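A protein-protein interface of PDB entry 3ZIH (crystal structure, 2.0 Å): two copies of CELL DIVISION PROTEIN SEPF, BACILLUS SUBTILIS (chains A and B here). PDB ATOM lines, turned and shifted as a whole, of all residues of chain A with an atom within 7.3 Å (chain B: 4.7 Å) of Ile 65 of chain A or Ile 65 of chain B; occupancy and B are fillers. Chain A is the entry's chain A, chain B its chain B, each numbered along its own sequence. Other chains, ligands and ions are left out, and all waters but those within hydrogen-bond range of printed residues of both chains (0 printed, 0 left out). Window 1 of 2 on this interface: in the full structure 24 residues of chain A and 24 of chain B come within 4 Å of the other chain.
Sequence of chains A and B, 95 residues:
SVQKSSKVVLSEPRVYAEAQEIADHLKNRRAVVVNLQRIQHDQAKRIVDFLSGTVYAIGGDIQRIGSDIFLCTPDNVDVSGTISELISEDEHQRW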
ATOM      1  N   LEU A  10       2.522  -6.884  29.940  1.00  0.00           N
ATOM      2  CA  LEU A  10       2.557  -8.276  30.368  1.00  0.00           C
ATOM      3  C   LEU A  10       1.098  -8.788  30.386  1.00  0.00           C
ATOM      4  O   LEU A  10       0.221  -8.181  30.998  1.00  0.00           O
ATOM      5  CB  LEU A  10       3.141  -8.470  31.748  1.00  0.00           C
ATOM      6  CG  LEU A  10       4.396  -7.684  32.080  1.00  0.00           C
ATOM      7  CD1 LEU A  10       4.774  -8.031  33.527  1.00  0.00           C
ATOM      8  CD2 LEU A  10       5.495  -8.040  31.086  1.00  0.00           C
ATOM      9  N   SER A  11       0.868  -9.916  29.742  1.00  0.00           N
ATOM     10  CA  SER A  11      -0.476 -10.478  29.619  1.00  0.00           C
ATOM     11  C   SER A  11      -0.411 -11.958  29.964  1.00  0.00           C
ATOM     12  O   SER A  11       0.556 -12.608  29.618  1.00  0.00           O
ATOM     13  CB  SER A  11      -0.917 -10.313  28.165  1.00  0.00           C
ATOM     14  OG  SER A  11      -2.181 -10.888  27.960  1.00  0.00           O
ATOM     15  N   GLU A  12      -1.409 -12.439  30.702  1.00  0.00           N
ATOM     16  CA  GLU A  12      -1.555 -13.823  31.064  1.00  0.00           C
ATOM     17  C   GLU A  12      -3.005 -14.162  30.740  1.00  0.00           C
ATOM     18  O   GLU A  12      -3.873 -14.203  31.621  1.00  0.00           O
ATOM     19  CB  GLU A  12      -1.285 -14.031  32.554  1.00  0.00           C
ATOM     20  CG  GLU A  12      -0.834 -15.418  32.962  1.00  0.00           C
ATOM     21  CD  GLU A  12      -0.596 -15.494  34.499  1.00  0.00           C
ATOM     22  OE1 GLU A  12      -1.075 -14.567  35.227  1.00  0.00           O
ATOM     23  OE2 GLU A  12       0.068 -16.458  34.963  1.00  0.00           O
ATOM     24  N   VAL A  32       4.155  -6.948  23.672  1.00  0.00           N
ATOM     25  CA  VAL A  32       3.415  -7.630  24.724  1.00  0.00           C
ATOM     26  C   VAL A  32       4.114  -8.978  24.982  1.00  0.00           C
ATOM     27  O   VAL A  32       4.400  -9.771  24.037  1.00  0.00           O
ATOM     28  CB  VAL A  32       1.954  -7.951  24.274  1.00  0.00           C
ATOM     29  CG1 VAL A  32       1.209  -8.607  25.402  1.00  0.00           C
ATOM     30  CG2 VAL A  32       1.245  -6.676  23.728  1.00  0.00           C
ATOM     31  N   VAL A  33       4.300  -9.259  26.252  1.00  0.00           N
ATOM     32  CA  VAL A  33       4.752 -10.577  26.681  1.00  0.00           C
ATOM     33  C   VAL A  33       3.502 -11.366  26.956  1.00  0.00           C
ATOM     34  O   VAL A  33       2.662 -10.914  27.752  1.00  0.00           O
ATOM     35  CB  VAL A  33       5.623 -10.481  27.988  1.00  0.00           C
ATOM     36  CG1 VAL A  33       5.932 -11.903  28.548  1.00  0.00           C
ATOM     37  CG2 VAL A  33       6.923  -9.774  27.676  1.00  0.00           C
ATOM     38  N   VAL A  34       3.386 -12.559  26.380  1.00  0.00           N
ATOM     39  CA  VAL A  34       2.143 -13.333  26.518  1.00  0.00           C
ATOM     40  C   VAL A  34       2.521 -14.614  27.198  1.00  0.00           C
ATOM     41  O   VAL A  34       3.238 -15.407  26.638  1.00  0.00           O
ATOM     42  CB  VAL A  34       1.435 -13.604  25.135  1.00  0.00           C
ATOM     43  CG1 VAL A  34       0.031 -14.374  25.377  1.00  0.00           C
ATOM     44  CG2 VAL A  34       1.291 -12.305  24.294  1.00  0.00           C
ATOM     45  N   ASN A  35       2.107 -14.775  28.437  1.00  0.00           N
ATOM     46  CA  ASN A  35       2.453 -15.937  29.223  1.00  0.00           C
ATOM     47  C   ASN A  35       1.209 -16.828  29.116  1.00  0.00           C
ATOM     48  O   ASN A  35       0.109 -16.388  29.527  1.00  0.00           O
ATOM     49  CB  ASN A  35       2.644 -15.537  30.690  1.00  0.00           C
ATOM     50  CG  ASN A  35       2.960 -16.734  31.559  1.00  0.00           C
ATOM     51  OD1 ASN A  35       2.264 -17.732  31.506  1.00  0.00           O
ATOM     52  ND2 ASN A  35       4.087 -16.699  32.245  1.00  0.00           N
ATOM     53  N   LEU A  36       1.372 -18.020  28.607  1.00  0.00           N
ATOM     54  CA  LEU A  36       0.216 -18.947  28.425  1.00  0.00           C
ATOM     55  C   LEU A  36       0.333 -20.151  29.362  1.00  0.00           C
ATOM     56  O   LEU A  36      -0.125 -21.267  29.062  1.00  0.00           O
ATOM     57  CB  LEU A  36       0.150 -19.414  26.962  1.00  0.00           C
ATOM     58  CG  LEU A  36      -0.033 -18.277  25.951  1.00  0.00           C
ATOM     59  CD1 LEU A  36       0.185 -18.719  24.418  1.00  0.00           C
ATOM     60  CD2 LEU A  36      -1.408 -17.695  26.154  1.00  0.00           C
ATOM     61  N   GLN A  37       0.885 -19.917  30.557  1.00  0.00           N
ATOM     62  CA  GLN A  37       1.145 -21.009  31.518  1.00  0.00           C
ATOM     63  C   GLN A  37      -0.103 -21.357  32.233  1.00  0.00           C
ATOM     64  O   GLN A  37      -0.258 -22.498  32.616  1.00  0.00           O
ATOM     65  CB  GLN A  37       2.283 -20.654  32.542  1.00  0.00           C
ATOM     66  CG  GLN A  37       3.682 -20.593  31.835  1.00  0.00           C
ATOM     67  CD  GLN A  37       4.896 -20.087  32.744  1.00  0.00           C
ATOM     68  OE1 GLN A  37       4.715 -19.578  33.856  1.00  0.00           O
ATOM     69  NE2 GLN A  37       6.107 -20.217  32.211  1.00  0.00           N
ATOM     70  N   GLN A  63       7.569 -14.381  18.801  1.00  0.00           N
ATOM     71  CA  GLN A  63       8.747 -15.225  19.119  1.00  0.00           C
ATOM     72  C   GLN A  63       8.512 -15.937  20.417  1.00  0.00           C
ATOM     73  O   GLN A  63       8.033 -15.308  21.372  1.00  0.00           O
ATOM     74  CB  GLN A  63       9.987 -14.387  19.383  1.00  0.00           C
ATOM     75  CG  GLN A  63      10.670 -13.872  18.220  1.00  0.00           C
ATOM     76  CD  GLN A  63      12.205 -13.903  18.408  1.00  0.00           C
ATOM     77  OE1 GLN A  63      12.772 -14.895  18.920  1.00  0.00           O
ATOM     78  NE2 GLN A  63      12.874 -12.836  17.972  1.00  0.00           N
ATOM     79  N   ARG A  64       8.800 -17.244  20.452  1.00  0.00           N
ATOM     80  CA  ARG A  64       8.651 -18.039  21.668  1.00  0.00           C
ATOM     81  C   ARG A  64       9.825 -17.646  22.541  1.00  0.00           C
ATOM     82  O   ARG A  64      10.953 -17.649  22.065  1.00  0.00           O
ATOM     83  CB  ARG A  64       8.724 -19.522  21.357  1.00  0.00           C
ATOM     84  CG  ARG A  64       8.539 -20.445  22.480  1.00  0.00           C
ATOM     85  CD  ARG A  64       8.507 -21.950  21.988  1.00  0.00           C
ATOM     86  NE  ARG A  64       7.335 -22.611  22.593  1.00  0.00           N
ATOM     87  CZ  ARG A  64       7.356 -23.489  23.609  1.00  0.00           C
ATOM     88  NH1 ARG A  64       8.510 -23.910  24.152  1.00  0.00           N
ATOM     89  NH2 ARG A  64       6.210 -23.958  24.099  1.00  0.00           N
ATOM     90  N   ILE A  65       9.574 -17.266  23.783  1.00  0.00           N
ATOM     91  CA  ILE A  65      10.715 -16.860  24.643  1.00  0.00           C
ATOM     92  C   ILE A  65      10.974 -17.795  25.854  1.00  0.00           C
ATOM     93  O   ILE A  65      11.923 -17.585  26.627  1.00  0.00           O
ATOM     94  CB  ILE A  65      10.637 -15.357  25.062  1.00  0.00           C
ATOM     95  CG1 ILE A  65       9.346 -15.060  25.806  1.00  0.00           C
ATOM     96  CG2 ILE A  65      10.908 -14.454  23.862  1.00  0.00           C
ATOM     97  CD1 ILE A  65       9.264 -13.659  26.491  1.00  0.00           C
ATOM     98  N   GLY A  66      10.150 -18.825  25.967  1.00  0.00           N
ATOM     99  CA  GLY A  66      10.299 -19.889  26.923  1.00  0.00           C
ATOM    100  C   GLY A  66       9.124 -20.820  26.744  1.00  0.00           C
ATOM    101  O   GLY A  66       8.377 -20.690  25.785  1.00  0.00           O
ATOM    102  N   SER A  67       8.955 -21.753  27.672  1.00  0.00           N
ATOM    103  CA  SER A  67       7.808 -22.683  27.641  1.00  0.00           C
ATOM    104  C   SER A  67       6.513 -21.964  27.790  1.00  0.00           C
ATOM    105  O   SER A  67       6.293 -21.372  28.808  1.00  0.00           O
ATOM    106  CB  SER A  67       7.877 -23.681  28.813  1.00  0.00           C
ATOM    107  OG  SER A  67       8.876 -24.603  28.486  1.00  0.00           O
ATOM    108  N   ASP A  68       5.639 -22.031  26.794  1.00  0.00           N
ATOM    109  CA  ASP A  68       4.321 -21.437  26.936  1.00  0.00           C
ATOM    110  C   ASP A  68       4.406 -19.885  27.093  1.00  0.00           C
ATOM    111  O   ASP A  68       3.563 -19.280  27.695  1.00  0.00           O
ATOM    112  CB  ASP A  68       3.593 -22.025  28.163  1.00  0.00           C
ATOM    113  CG  ASP A  68       3.719 -23.580  28.280  1.00  0.00           C
ATOM    114  OD1 ASP A  68       3.599 -24.261  27.210  1.00  0.00           O
ATOM    115  OD2 ASP A  68       3.924 -24.091  29.457  1.00  0.00           O
ATOM    116  N   ILE A  69       5.472 -19.284  26.626  1.00  0.00           N
ATOM    117  CA  ILE A  69       5.640 -17.831  26.701  1.00  0.00           C
ATOM    118  C   ILE A  69       6.199 -17.255  25.437  1.00  0.00           C
ATOM    119  O   ILE A  69       7.220 -17.729  24.877  1.00  0.00           O
ATOM    120  CB  ILE A  69       6.457 -17.356  27.949  1.00  0.00           C
ATOM    121  CG1 ILE A  69       6.460 -15.822  28.041  1.00  0.00           C
ATOM    122  CG2 ILE A  69       7.826 -17.938  27.924  1.00  0.00           C
ATOM    123  CD1 ILE A  69       6.537 -15.322  29.465  1.00  0.00           C
ATOM    124  N   PHE A  70       5.525 -16.180  25.026  1.00  0.00           N
ATOM    125  CA  PHE A  70       5.792 -15.513  23.758  1.00  0.00           C
ATOM    126  C   PHE A  70       5.956 -14.016  23.863  1.00  0.00           C
ATOM    127  O   PHE A  70       5.311 -13.358  24.717  1.00  0.00           O
ATOM    128  CB  PHE A  70       4.606 -15.816  22.801  1.00  0.00           C
ATOM    129  CG  PHE A  70       4.511 -17.243  22.468  1.00  0.00           C
ATOM    130  CD1 PHE A  70       3.851 -18.124  23.324  1.00  0.00           C
ATOM    131  CD2 PHE A  70       5.182 -17.742  21.337  1.00  0.00           C
ATOM    132  CE1 PHE A  70       3.832 -19.490  23.051  1.00  0.00           C
ATOM    133  CE2 PHE A  70       5.131 -19.114  21.073  1.00  0.00           C
ATOM    134  CZ  PHE A  70       4.489 -19.970  21.922  1.00  0.00           C
ATOM    135  N   LEU A  71       6.787 -13.475  22.971  1.00  0.00           N
ATOM    136  CA  LEU A  71       6.983 -12.060  22.860  1.00  0.00           C
ATOM    137  C   LEU A  71       6.368 -11.640  21.528  1.00  0.00           C
ATOM    138  O   LEU A  71       6.788 -12.113  20.471  1.00  0.00           O
ATOM    139  CB  LEU A  71       8.474 -11.694  22.905  1.00  0.00           C
ATOM    140  CG  LEU A  71       8.736 -10.161  22.726  1.00  0.00           C
ATOM    141  CD1 LEU A  71       8.028  -9.279  23.827  1.00  0.00           C
ATOM    142  CD2 LEU A  71      10.239  -9.903  22.612  1.00  0.00           C
ATOM    143  N   CYS A  72       5.312 -10.840  21.585  1.00  0.00           N
ATOM    144  CA  CYS A  72       4.791 -10.222  20.371  1.00  0.00           C
ATOM    145  C   CYS A  72       5.237  -8.779  20.276  1.00  0.00           C
ATOM    146  O   CYS A  72       5.190  -8.026  21.230  1.00  0.00           O
ATOM    147  CB  CYS A  72       3.299 -10.286  20.323  1.00  0.00           C
ATOM    148  SG  CYS A  72       2.567 -11.940  20.574  1.00  0.00           S
ATOM    149  N   VAL A  79      13.825  -6.864  17.950  1.00  0.00           N
ATOM    150  CA  VAL A  79      14.198  -7.902  18.913  1.00  0.00           C
ATOM    151  C   VAL A  79      15.533  -8.483  18.454  1.00  0.00           C
ATOM    152  O   VAL A  79      15.689  -8.778  17.260  1.00  0.00           O
ATOM    153  CB  VAL A  79      13.120  -9.005  18.981  1.00  0.00           C
ATOM    154  CG1 VAL A  79      13.479 -10.109  20.013  1.00  0.00           C
ATOM    155  CG2 VAL A  79      11.774  -8.390  19.416  1.00  0.00           C
ATOM    156  N   ILE A  83      16.540 -17.609  21.726  1.00  0.00           N
ATOM    157  CA  ILE A  83      16.308 -18.418  22.913  1.00  0.00           C
ATOM    158  C   ILE A  83      16.118 -19.894  22.506  1.00  0.00           C
ATOM    159  O   ILE A  83      15.118 -20.234  21.879  1.00  0.00           O
ATOM    160  CB  ILE A  83      15.104 -17.785  23.767  1.00  0.00           C
ATOM    161  CG1 ILE A  83      15.639 -16.534  24.516  1.00  0.00           C
ATOM    162  CG2 ILE A  83      14.456 -18.840  24.700  1.00  0.00           C
ATOM    163  CD1 ILE A  83      14.740 -15.905  25.555  1.00  0.00           C
ATOM    164  N   LEU B  10      16.926 -10.756  23.749  1.00  0.00           N
ATOM    165  CA  LEU B  10      16.565 -12.014  24.296  1.00  0.00           C
ATOM    166  C   LEU B  10      17.832 -12.680  24.714  1.00  0.00           C
ATOM    167  O   LEU B  10      18.773 -12.772  23.913  1.00  0.00           O
ATOM    168  CB  LEU B  10      15.891 -12.902  23.279  1.00  0.00           C
ATOM    169  CG  LEU B  10      14.714 -12.295  22.532  1.00  0.00           C
ATOM    170  CD1 LEU B  10      14.183 -13.383  21.456  1.00  0.00           C
ATOM    171  CD2 LEU B  10      13.663 -11.929  23.556  1.00  0.00           C
ATOM    172  N   VAL B  33      15.000  -9.738  28.007  1.00  0.00           N
ATOM    173  CA  VAL B  33      14.325 -10.926  28.442  1.00  0.00           C
ATOM    174  C   VAL B  33      15.383 -11.946  28.817  1.00  0.00           C
ATOM    175  O   VAL B  33      16.243 -12.266  27.988  1.00  0.00           O
ATOM    176  CB  VAL B  33      13.398 -11.498  27.349  1.00  0.00           C
ATOM    177  CG1 VAL B  33      12.893 -12.886  27.755  1.00  0.00           C
ATOM    178  CG2 VAL B  33      12.198 -10.536  27.082  1.00  0.00           C
ATOM    179  N   ASN B  35      15.901 -15.732  30.012  1.00  0.00           N
ATOM    180  CA  ASN B  35      15.308 -17.059  30.149  1.00  0.00           C
ATOM    181  C   ASN B  35      16.304 -17.924  30.910  1.00  0.00           C
ATOM    182  O   ASN B  35      17.404 -18.091  30.437  1.00  0.00           O
ATOM    183  CB  ASN B  35      15.045 -17.663  28.777  1.00  0.00           C
ATOM    184  CG  ASN B  35      14.443 -19.041  28.863  1.00  0.00           C
ATOM    185  OD1 ASN B  35      14.785 -19.800  29.744  1.00  0.00           O
ATOM    186  ND2 ASN B  35      13.504 -19.342  28.003  1.00  0.00           N
ATOM    187  N   GLN B  63      11.477  -8.286  36.806  1.00  0.00           N
ATOM    188  CA  GLN B  63      10.138  -8.817  37.122  1.00  0.00           C
ATOM    189  C   GLN B  63      10.036 -10.231  36.548  1.00  0.00           C
ATOM    190  O   GLN B  63      10.462 -10.454  35.419  1.00  0.00           O
ATOM    191  CB  GLN B  63       9.145  -7.835  36.511  1.00  0.00           C
ATOM    192  CG  GLN B  63       7.778  -8.070  36.806  1.00  0.00           C
ATOM    193  CD  GLN B  63       6.860  -6.904  36.332  1.00  0.00           C
ATOM    194  OE1 GLN B  63       7.299  -5.820  35.930  1.00  0.00           O
ATOM    195  NE2 GLN B  63       5.584  -7.152  36.416  1.00  0.00           N
ATOM    196  N   ARG B  64       9.540 -11.185  37.345  1.00  0.00           N
ATOM    197  CA  ARG B  64       9.286 -12.539  36.879  1.00  0.00           C
ATOM    198  C   ARG B  64       8.168 -12.513  35.838  1.00  0.00           C
ATOM    199  O   ARG B  64       7.130 -11.898  36.079  1.00  0.00           O
ATOM    200  CB  ARG B  64       8.849 -13.444  38.021  1.00  0.00           C
ATOM    201  CG  ARG B  64       8.882 -14.911  37.689  1.00  0.00           C
ATOM    202  CD  ARG B  64       8.711 -15.712  38.983  1.00  0.00           C
ATOM    203  NE  ARG B  64       8.296 -17.101  38.759  1.00  0.00           N
ATOM    204  CZ  ARG B  64       7.095 -17.508  38.283  1.00  0.00           C
ATOM    205  NH1 ARG B  64       6.131 -16.642  37.931  1.00  0.00           N
ATOM    206  NH2 ARG B  64       6.855 -18.831  38.162  1.00  0.00           N
ATOM    207  N   ILE B  65       8.425 -13.080  34.659  1.00  0.00           N
ATOM    208  CA  ILE B  65       7.347 -13.132  33.600  1.00  0.00           C
ATOM    209  C   ILE B  65       6.837 -14.552  33.324  1.00  0.00           C
ATOM    210  O   ILE B  65       5.968 -14.782  32.463  1.00  0.00           O
ATOM    211  CB  ILE B  65       7.703 -12.376  32.331  1.00  0.00           C
ATOM    212  CG1 ILE B  65       8.893 -12.984  31.638  1.00  0.00           C
ATOM    213  CG2 ILE B  65       7.744 -10.847  32.640  1.00  0.00           C
ATOM    214  CD1 ILE B  65       9.232 -12.301  30.197  1.00  0.00           C
ATOM    215  N   GLY B  66       7.375 -15.504  34.062  1.00  0.00           N
ATOM    216  CA  GLY B  66       6.941 -16.891  33.958  1.00  0.00           C
ATOM    217  C   GLY B  66       7.954 -17.713  34.749  1.00  0.00           C
ATOM    218  O   GLY B  66       8.806 -17.148  35.476  1.00  0.00           O
ATOM    219  N   ILE B  69      11.774 -17.267  34.136  1.00  0.00           N
ATOM    220  CA  ILE B  69      12.029 -16.233  33.140  1.00  0.00           C
ATOM    221  C   ILE B  69      11.637 -14.827  33.661  1.00  0.00           C
ATOM    222  O   ILE B  69      10.587 -14.630  34.299  1.00  0.00           O
ATOM    223  CB  ILE B  69      11.338 -16.622  31.809  1.00  0.00           C
ATOM    224  CG1 ILE B  69      11.515 -15.519  30.767  1.00  0.00           C
ATOM    225  CG2 ILE B  69       9.870 -16.996  32.073  1.00  0.00           C
ATOM    226  CD1 ILE B  69      11.141 -15.967  29.390  1.00  0.00           C
ATOM    227  N   PHE B  70      12.501 -13.867  33.341  1.00  0.00           N
ATOM    228  CA  PHE B  70      12.406 -12.492  33.850  1.00  0.00           C
ATOM    229  C   PHE B  70      12.545 -11.481  32.757  1.00  0.00           C
ATOM    230  O   PHE B  70      13.227 -11.705  31.782  1.00  0.00           O
ATOM    231  CB  PHE B  70      13.547 -12.266  34.860  1.00  0.00           C
ATOM    232  CG  PHE B  70      13.499 -13.238  35.993  1.00  0.00           C
ATOM    233  CD1 PHE B  70      13.984 -14.541  35.823  1.00  0.00           C
ATOM    234  CD2 PHE B  70      12.891 -12.895  37.177  1.00  0.00           C
ATOM    235  CE1 PHE B  70      13.866 -15.495  36.851  1.00  0.00           C
ATOM    236  CE2 PHE B  70      12.798 -13.828  38.213  1.00  0.00           C
ATOM    237  CZ  PHE B  70      13.272 -15.131  38.040  1.00  0.00           C
ATOM    238  N   LEU B  71      11.953 -10.339  32.977  1.00  0.00           N
ATOM    239  CA  LEU B  71      12.148  -9.173  32.155  1.00  0.00           C
ATOM    240  C   LEU B  71      12.901  -8.133  33.015  1.00  0.00           C
ATOM    241  O   LEU B  71      12.400  -7.749  34.098  1.00  0.00           O
ATOM    242  CB  LEU B  71      10.801  -8.609  31.730  1.00  0.00           C
ATOM    243  CG  LEU B  71      10.837  -7.249  30.976  1.00  0.00           C
ATOM    244  CD1 LEU B  71      11.539  -7.446  29.640  1.00  0.00           C
ATOM    245  CD2 LEU B  71       9.367  -6.763  30.798  1.00  0.00           C
ATOM    246  N   ILE B  83       1.848 -10.939  35.941  1.00  0.00           N
ATOM    247  CA  ILE B  83       1.893 -12.353  35.702  1.00  0.00           C
ATOM    248  C   ILE B  83       2.007 -13.022  37.074  1.00  0.00           C
ATOM    249  O   ILE B  83       2.956 -12.779  37.820  1.00  0.00           O
ATOM    250  CB  ILE B  83       3.090 -12.721  34.791  1.00  0.00           C
ATOM    251  CG1 ILE B  83       2.711 -12.477  33.317  1.00  0.00           C
ATOM    252  CG2 ILE B  83       3.538 -14.155  35.045  1.00  0.00           C
ATOM    253  CD1 ILE B  83       3.886 -12.536  32.329  1.00  0.00           C
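The backbone carbonyl oxygen (O) of Ile 65 of chain B is in hydrogen-bond range of the side-chain amide nitrogen (ND2) of Asn 35 of chain A (2.7 Å). O of Ile 65 of chain A sits at hydrogen-bond distance from ND2 of Asn 35 of chain B, at 2.7 Å.
The backbone carbonyl oxygen (O) of Val 33 of chain A sits at hydrogen-bond distance from the backbone NH (N) of Ser 11 of chain A (2.9 Å). The backbone NH of Asn 35 of chain A sits at hydrogen-bond distance from the backbone carbonyl oxygen of Ser 11 of chain A, 2.9 Å away. OD1 of Asn 35 of chain A is in hydrogen-bond range of N of Gln 37 of chain A, 2.8 Å away. O of Gln 63 of chain A sits at hydrogen-bond distance from N of Leu 71 of chain A, 2.7 Å away. O of Gln 63 of chain B sits at hydrogen-bond distance from N of Leu 71 of chain B, 2.9 Å away. The backbone carbonyl oxygen of Gly 66 of chain B lies close to the guanidinium group of Arg 64 of chain B (3.3 Å).
Ile 83 of chain B touches Glu 12 of chain A. CD1 of Ile 65 of chain B touches CG1 of Val 33 of chain A (3.7 Å). ND2 of Asn 35 of chain A touches CA of Gly 66 of chain B (3.3 Å). Asn 35 of chain A touches Ile 83 of chain B. CG2 of Ile 65 of chain A touches CD2 of Leu 10 of chain B (3.7 Å). Ile 65 of chain B touches Ile 65 of chain A (CD1 to CD1, 3.9 Å). Asn 35 of chain B touches Gly 66 of chain A (ND2 to CA, 3.4 Å). CG of Leu 10 of chain B touches CG1 of Val 79 of chain A, at 3.6 Å. Leu 10 of chain B touches Ile 83 of chain A. Ile 83 of chain A touches Asn 35 of chain B (CG2 to ND2, 3.5 Å).
Of chain B, only Leu 10, Val 33, Asn 35, Ile 65 and Ile 69 come within 4 Å of Ile 65 of chain A. Ile 65 of chain B touches five residues of chain A. Of the printed residues of chain B, Glu 12 of chain A touches Ile 83. Of the printed residues of chain B, Gln 63 of chain A touches Leu 10 (3.3 Å). Printed residues of chain B within 4 Å of Ile 83 of chain A: Leu 10 and Asn 35. Phe 70 of chain A touches none of the printed residues of chain B. The nearest printed residue of chain B that does not touch Ile 65 of chain A is Phe 70 of chain B (6.9 Å). The nearest residue of chain A that does not touch Ile 65 of chain B is Gln 37 of chain A (5.1 Å).
Of the 21 printed residues of chain A, 11 touch a printed residue of chain B. Hydrophobic or aromatic side chains of chain A that line the printed part of chain B: Leu 10, Val 33, Ile 65, Ile 69, Val 79 and Ile 83. Of the 11 printed residues of chain B, 8 touch a printed residue of chain A. Hydrophobic or aromatic side chains of chain B within 4 Å of the printed part of chain A: Leu 10, Val 33, Ile 65, Ile 69 and Ile 83. Along chain B the printed residues that touch a printed residue of chain A span positions 10 to 83. Among the printed residues, 19 pairs touch across the chains. Among the printed residues, no Asp or Glu carboxylate lies within 4 Å of a Lys or Arg side-chain nitrogen of the other chain.
Val 33 of chain A touches Ile 65 of chain B, and with the chains exchanged Ile 65 of chain A touches Val 33 of chain B. Asn 35 of chain A touches Ile 65 of chain B, and with the chains exchanged Ile 65 of chain A touches Asn 35 of chain B. Asn 35 of chain A touches Gly 66 of chain B, and with the chains exchanged Gly 66 of chain A touches Asn 35 of chain B. Asn 35 of chain A touches Ile 83 of chain B, and with the chains exchanged Ile 83 of chain A touches Asn 35 of chain B.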
